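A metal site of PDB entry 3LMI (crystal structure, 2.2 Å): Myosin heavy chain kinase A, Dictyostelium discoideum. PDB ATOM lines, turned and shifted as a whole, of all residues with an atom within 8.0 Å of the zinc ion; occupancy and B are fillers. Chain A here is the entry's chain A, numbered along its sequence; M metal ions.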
ATOM      1  N   SER A 201     -29.264 -16.483   6.922  1.00  0.00           N
ATOM      2  CA  SER A 201     -29.028 -16.956   5.560  1.00  0.00           C
ATOM      3  C   SER A 201     -27.573 -16.770   5.109  1.00  0.00           C
ATOM      4  O   SER A 201     -26.993 -17.645   4.463  1.00  0.00           O
ATOM      5  CB  SER A 201     -29.930 -16.195   4.570  1.00  0.00           C
ATOM      6  OG  SER A 201     -31.243 -16.721   4.537  1.00  0.00           O
ATOM      7  N   GLN A 204     -24.776 -19.518   5.768  1.00  0.00           N
ATOM      8  CA  GLN A 204     -24.913 -20.799   5.040  1.00  0.00           C
ATOM      9  C   GLN A 204     -24.688 -20.651   3.538  1.00  0.00           C
ATOM     10  O   GLN A 204     -24.183 -21.580   2.896  1.00  0.00           O
ATOM     11  CB  GLN A 204     -26.274 -21.475   5.304  1.00  0.00           C
ATOM     12  CG  GLN A 204     -26.675 -21.631   6.779  1.00  0.00           C
ATOM     13  CD  GLN A 204     -25.647 -22.387   7.618  1.00  0.00           C
ATOM     14  OE1 GLN A 204     -25.071 -23.392   7.184  1.00  0.00           O
ATOM     15  NE2 GLN A 204     -25.432 -21.914   8.837  1.00  0.00           N
ATOM     16  N   ALA A 205     -25.059 -19.508   2.996  1.00  0.00           N
ATOM     17  CA  ALA A 205     -24.857 -19.201   1.579  1.00  0.00           C
ATOM     18  C   ALA A 205     -23.376 -19.017   1.253  1.00  0.00           C
ATOM     19  O   ALA A 205     -22.926 -19.376   0.164  1.00  0.00           O
ATOM     20  CB  ALA A 205     -25.672 -17.956   1.168  1.00  0.00           C
ATOM     21  N   PHE A 206     -22.635 -18.439   2.201  1.00  0.00           N
ATOM     22  CA  PHE A 206     -21.196 -18.278   2.020  1.00  0.00           C
ATOM     23  C   PHE A 206     -20.521 -19.643   1.930  1.00  0.00           C
ATOM     24  O   PHE A 206     -19.714 -19.887   1.014  1.00  0.00           O
ATOM     25  CB  PHE A 206     -20.557 -17.443   3.134  1.00  0.00           C
ATOM     26  CG  PHE A 206     -19.030 -17.488   3.120  1.00  0.00           C
ATOM     27  CD1 PHE A 206     -18.298 -16.762   2.188  1.00  0.00           C
ATOM     28  CD2 PHE A 206     -18.338 -18.283   4.044  1.00  0.00           C
ATOM     29  CE1 PHE A 206     -16.905 -16.792   2.174  1.00  0.00           C
ATOM     30  CE2 PHE A 206     -16.934 -18.318   4.051  1.00  0.00           C
ATOM     31  CZ  PHE A 206     -16.214 -17.576   3.111  1.00  0.00           C
ATOM     32  N   SER A 207     -20.839 -20.535   2.861  1.00  0.00           N
ATOM     33  CA  SER A 207     -20.293 -21.895   2.781  1.00  0.00           C
ATOM     34  C   SER A 207     -20.528 -22.521   1.412  1.00  0.00           C
ATOM     35  O   SER A 207     -19.584 -22.976   0.757  1.00  0.00           O
ATOM     36  CB  SER A 207     -20.852 -22.791   3.893  1.00  0.00           C
ATOM     37  OG  SER A 207     -20.333 -22.412   5.144  1.00  0.00           O
ATOM     38  N   HIS A 208     -21.789 -22.548   0.970  1.00  0.00           N
ATOM     39  CA  HIS A 208     -22.161 -23.113  -0.330  1.00  0.00           C
ATOM     40  C   HIS A 208     -21.346 -22.456  -1.470  1.00  0.00           C
ATOM     41  O   HIS A 208     -20.765 -23.138  -2.317  1.00  0.00           O
ATOM     42  CB  HIS A 208     -23.684 -22.950  -0.539  1.00  0.00           C
ATOM     43  CG  HIS A 208     -24.221 -23.646  -1.743  1.00  0.00           C
ATOM     44  ND1 HIS A 208     -25.547 -23.589  -2.106  1.00  0.00           N
ATOM     45  CD2 HIS A 208     -23.608 -24.397  -2.701  1.00  0.00           C
ATOM     46  CE1 HIS A 208     -25.743 -24.283  -3.218  1.00  0.00           C
ATOM     47  NE2 HIS A 208     -24.575 -24.792  -3.597  1.00  0.00           N
ATOM     48  N   PHE A 209     -21.306 -21.129  -1.466  1.00  0.00           N
ATOM     49  CA  PHE A 209     -20.490 -20.343  -2.400  1.00  0.00           C
ATOM     50  C   PHE A 209     -19.044 -20.890  -2.558  1.00  0.00           C
ATOM     51  O   PHE A 209     -18.580 -21.101  -3.683  1.00  0.00           O
ATOM     52  CB  PHE A 209     -20.536 -18.849  -1.968  1.00  0.00           C
ATOM     53  CG  PHE A 209     -19.695 -17.926  -2.827  1.00  0.00           C
ATOM     54  CD1 PHE A 209     -20.256 -17.292  -3.940  1.00  0.00           C
ATOM     55  CD2 PHE A 209     -18.373 -17.659  -2.501  1.00  0.00           C
ATOM     56  CE1 PHE A 209     -19.513 -16.449  -4.719  1.00  0.00           C
ATOM     57  CE2 PHE A 209     -17.613 -16.774  -3.282  1.00  0.00           C
ATOM     58  CZ  PHE A 209     -18.177 -16.185  -4.383  1.00  0.00           C
ATOM     59  N   GLU A 212     -18.988 -24.385  -4.427  1.00  0.00           N
ATOM     60  CA  GLU A 212     -19.293 -24.313  -5.857  1.00  0.00           C
ATOM     61  C   GLU A 212     -18.221 -23.591  -6.668  1.00  0.00           C
ATOM     62  O   GLU A 212     -17.745 -24.111  -7.671  1.00  0.00           O
ATOM     63  CB  GLU A 212     -20.672 -23.707  -6.142  1.00  0.00           C
ATOM     64  CG  GLU A 212     -20.995 -23.673  -7.641  1.00  0.00           C
ATOM     65  CD  GLU A 212     -22.474 -23.408  -7.951  1.00  0.00           C
ATOM     66  OE1 GLU A 212     -23.335 -23.960  -7.235  1.00  0.00           O
ATOM     67  OE2 GLU A 212     -22.754 -22.671  -8.921  1.00  0.00           O
ATOM     68  N   PHE A 256     -21.782 -31.531   5.376  1.00  0.00           N
ATOM     69  CA  PHE A 256     -22.356 -30.224   5.027  1.00  0.00           C
ATOM     70  C   PHE A 256     -23.459 -30.378   3.986  1.00  0.00           C
ATOM     71  O   PHE A 256     -24.494 -29.724   4.066  1.00  0.00           O
ATOM     72  CB  PHE A 256     -21.303 -29.222   4.516  1.00  0.00           C
ATOM     73  CG  PHE A 256     -21.904 -27.905   4.075  1.00  0.00           C
ATOM     74  CD1 PHE A 256     -22.132 -26.873   4.993  1.00  0.00           C
ATOM     75  CD2 PHE A 256     -22.293 -27.703   2.751  1.00  0.00           C
ATOM     76  CE1 PHE A 256     -22.702 -25.666   4.596  1.00  0.00           C
ATOM     77  CE2 PHE A 256     -22.867 -26.486   2.336  1.00  0.00           C
ATOM     78  CZ  PHE A 256     -23.084 -25.472   3.272  1.00  0.00           C
ATOM     79  N   HIS A 260     -27.688 -28.977   4.204  1.00  0.00           N
ATOM     80  CA  HIS A 260     -27.800 -27.651   3.604  1.00  0.00           C
ATOM     81  C   HIS A 260     -29.128 -27.428   2.862  1.00  0.00           C
ATOM     82  O   HIS A 260     -29.530 -28.224   2.030  1.00  0.00           O
ATOM     83  CB  HIS A 260     -26.626 -27.338   2.672  1.00  0.00           C
ATOM     84  CG  HIS A 260     -26.732 -25.988   2.016  1.00  0.00           C
ATOM     85  ND1 HIS A 260     -26.549 -24.811   2.709  1.00  0.00           N
ATOM     86  CD2 HIS A 260     -27.051 -25.635   0.744  1.00  0.00           C
ATOM     87  CE1 HIS A 260     -26.715 -23.795   1.879  1.00  0.00           C
ATOM     88  NE2 HIS A 260     -27.031 -24.266   0.682  1.00  0.00           N
ATOM     89  N   LYS A 261     -29.786 -26.309   3.166  1.00  0.00           N
ATOM     90  CA  LYS A 261     -30.966 -25.886   2.431  1.00  0.00           C
ATOM     91  C   LYS A 261     -30.721 -24.463   1.899  1.00  0.00           C
ATOM     92  O   LYS A 261     -30.489 -23.518   2.670  1.00  0.00           O
ATOM     93  CB  LYS A 261     -32.199 -25.929   3.352  1.00  0.00           C
ATOM     94  CG  LYS A 261     -33.423 -25.201   2.817  1.00  0.00           C
ATOM     95  CD  LYS A 261     -34.120 -26.011   1.743  1.00  0.00           C
ATOM     96  CE  LYS A 261     -35.112 -25.162   0.974  1.00  0.00           C
ATOM     97  NZ  LYS A 261     -36.109 -26.016   0.252  1.00  0.00           N
ATOM     98  N   CYS A 262     -30.765 -24.291   0.591  1.00  0.00           N
ATOM     99  CA  CYS A 262     -30.406 -22.980   0.050  1.00  0.00           C
ATOM    100  C   CYS A 262     -31.499 -21.969   0.369  1.00  0.00           C
ATOM    101  O   CYS A 262     -32.662 -22.329   0.571  1.00  0.00           O
ATOM    102  CB  CYS A 262     -30.097 -23.053  -1.442  1.00  0.00           C
ATOM    103  SG  CYS A 262     -31.516 -23.541  -2.363  1.00  0.00           S
ATOM    104  N   ASN A 263     -31.113 -20.702   0.444  1.00  0.00           N
ATOM    105  CA  ASN A 263     -31.996 -19.653   0.930  1.00  0.00           C
ATOM    106  C   ASN A 263     -32.054 -18.549  -0.110  1.00  0.00           C
ATOM    107  O   ASN A 263     -31.639 -18.762  -1.249  1.00  0.00           O
ATOM    108  CB  ASN A 263     -31.482 -19.139   2.274  1.00  0.00           C
ATOM    109  CG  ASN A 263     -29.985 -18.887   2.256  1.00  0.00           C
ATOM    110  OD1 ASN A 263     -29.500 -18.062   1.492  1.00  0.00           O
ATOM    111  ND2 ASN A 263     -29.239 -19.601   3.108  1.00  0.00           N
ATOM    112  N   ALA A 264     -32.543 -17.381   0.268  1.00  0.00           N
ATOM    113  CA  ALA A 264     -32.700 -16.290  -0.701  1.00  0.00           C
ATOM    114  C   ALA A 264     -31.337 -15.758  -1.132  1.00  0.00           C
ATOM    115  O   ALA A 264     -31.200 -15.189  -2.214  1.00  0.00           O
ATOM    116  CB  ALA A 264     -33.571 -15.172  -0.121  1.00  0.00           C
ATOM    117  N   VAL A 265     -30.327 -15.940  -0.279  1.00  0.00           N
ATOM    118  CA  VAL A 265     -28.982 -15.497  -0.644  1.00  0.00           C
ATOM    119  C   VAL A 265     -28.340 -16.488  -1.641  1.00  0.00           C
ATOM    120  O   VAL A 265     -27.731 -16.069  -2.625  1.00  0.00           O
ATOM    121  CB  VAL A 265     -28.091 -15.213   0.582  1.00  0.00           C
ATOM    122  CG1 VAL A 265     -26.751 -14.633   0.128  1.00  0.00           C
ATOM    123  CG2 VAL A 265     -28.787 -14.241   1.530  1.00  0.00           C
ATOM    124  N   CYS A 266     -28.490 -17.787  -1.395  1.00  0.00           N
ATOM    125  CA  CYS A 266     -28.110 -18.782  -2.406  1.00  0.00           C
ATOM    126  C   CYS A 266     -28.727 -18.431  -3.775  1.00  0.00           C
ATOM    127  O   CYS A 266     -28.045 -18.468  -4.810  1.00  0.00           O
ATOM    128  CB  CYS A 266     -28.518 -20.207  -1.980  1.00  0.00           C
ATOM    129  SG  CYS A 266     -27.674 -20.982  -0.519  1.00  0.00           S
ATOM    130  N   ALA A 267     -30.004 -18.080  -3.778  1.00  0.00           N
ATOM    131  CA  ALA A 267     -30.708 -17.737  -5.035  1.00  0.00           C
ATOM    132  C   ALA A 267     -30.214 -16.430  -5.676  1.00  0.00           C
ATOM    133  O   ALA A 267     -29.893 -16.413  -6.867  1.00  0.00           O
ATOM    134  CB  ALA A 267     -32.216 -17.694  -4.805  1.00  0.00           C
ATOM    135  N   LEU A 271     -26.597 -19.804  -7.250  1.00  0.00           N
ATOM    136  CA  LEU A 271     -25.943 -21.084  -7.001  1.00  0.00           C
ATOM    137  C   LEU A 271     -26.879 -22.254  -7.333  1.00  0.00           C
ATOM    138  O   LEU A 271     -28.101 -22.113  -7.305  1.00  0.00           O
ATOM    139  CB  LEU A 271     -25.487 -21.183  -5.542  1.00  0.00           C
ATOM    140  CG  LEU A 271     -24.618 -20.036  -5.016  1.00  0.00           C
ATOM    141  CD1 LEU A 271     -24.403 -20.193  -3.516  1.00  0.00           C
ATOM    142  CD2 LEU A 271     -23.276 -19.965  -5.760  1.00  0.00           C
ATOM    143  N   ASP A 272     -26.295 -23.413  -7.630  1.00  0.00           N
ATOM    144  CA  ASP A 272     -27.072 -24.600  -8.001  1.00  0.00           C
ATOM    145  C   ASP A 272     -27.750 -25.247  -6.797  1.00  0.00           C
ATOM    146  O   ASP A 272     -27.100 -25.523  -5.788  1.00  0.00           O
ATOM    147  CB  ASP A 272     -26.144 -25.618  -8.682  1.00  0.00           C
ATOM    148  CG  ASP A 272     -26.888 -26.859  -9.161  1.00  0.00           C
ATOM    149  OD1 ASP A 272     -28.076 -26.760  -9.525  1.00  0.00           O
ATOM    150  OD2 ASP A 272     -26.264 -27.940  -9.177  1.00  0.00           O
ATOM    151  N   VAL A 273     -29.053 -25.504  -6.895  1.00  0.00           N
ATOM    152  CA  VAL A 273     -29.775 -26.205  -5.815  1.00  0.00           C
ATOM    153  C   VAL A 273     -29.283 -27.652  -5.629  1.00  0.00           C
ATOM    154  O   VAL A 273     -29.455 -28.236  -4.573  1.00  0.00           O
ATOM    155  CB  VAL A 273     -31.310 -26.228  -6.026  1.00  0.00           C
ATOM    156  CG1 VAL A 273     -31.821 -24.869  -6.493  1.00  0.00           C
ATOM    157  CG2 VAL A 273     -31.692 -27.328  -7.020  1.00  0.00           C
ATOM    158  N   LYS A 274     -28.667 -28.218  -6.658  1.00  0.00           N
ATOM    159  CA  LYS A 274     -28.163 -29.591  -6.571  1.00  0.00           C
ATOM    160  C   LYS A 274     -26.958 -29.727  -5.631  1.00  0.00           C
ATOM    161  O   LYS A 274     -25.811 -29.511  -6.033  1.00  0.00           O
ATOM    162  CB  LYS A 274     -27.831 -30.151  -7.959  1.00  0.00           C
ATOM    163  CG  LYS A 274     -29.042 -30.210  -8.891  1.00  0.00           C
ATOM    164  CD  LYS A 274     -28.770 -31.053 -10.120  1.00  0.00           C
ATOM    165  CE  LYS A 274     -30.056 -31.370 -10.868  1.00  0.00           C
ATOM    166  NZ  LYS A 274     -29.848 -32.466 -11.860  1.00  0.00           N
HETATM  167 ZN    ZN M   1     -27.290 -23.002  -1.011  1.00  0.00          ZN
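The backbone carbonyl oxygen (O) of Cys 266 lies within hydrogen-bond range of the backbone NH (N) of Leu 271 (3.1 Å).
The backbone NH of Cys 266 lies within hydrogen-bond range of the side-chain amide oxygen of Asn 263, 3.1 Å away.
A ring nitrogen (NE2) of His 208 lies close to the backbone carbonyl oxygen of Asp 272.
Merely in contact with the zinc ion: Cys 262 (2.8 Å).
Of the 21 residues printed, 4 come within 4 Å of the zinc ion.
The zinc ion is bound by the side-chain sulfur of Cys 266 (2.1 Å), a ring nitrogen (NE2) of His 260 (2.1 Å) and a ring nitrogen (ND1) of His 208 (2.1 Å).
The zinc ion has three donor atoms within binding distance.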
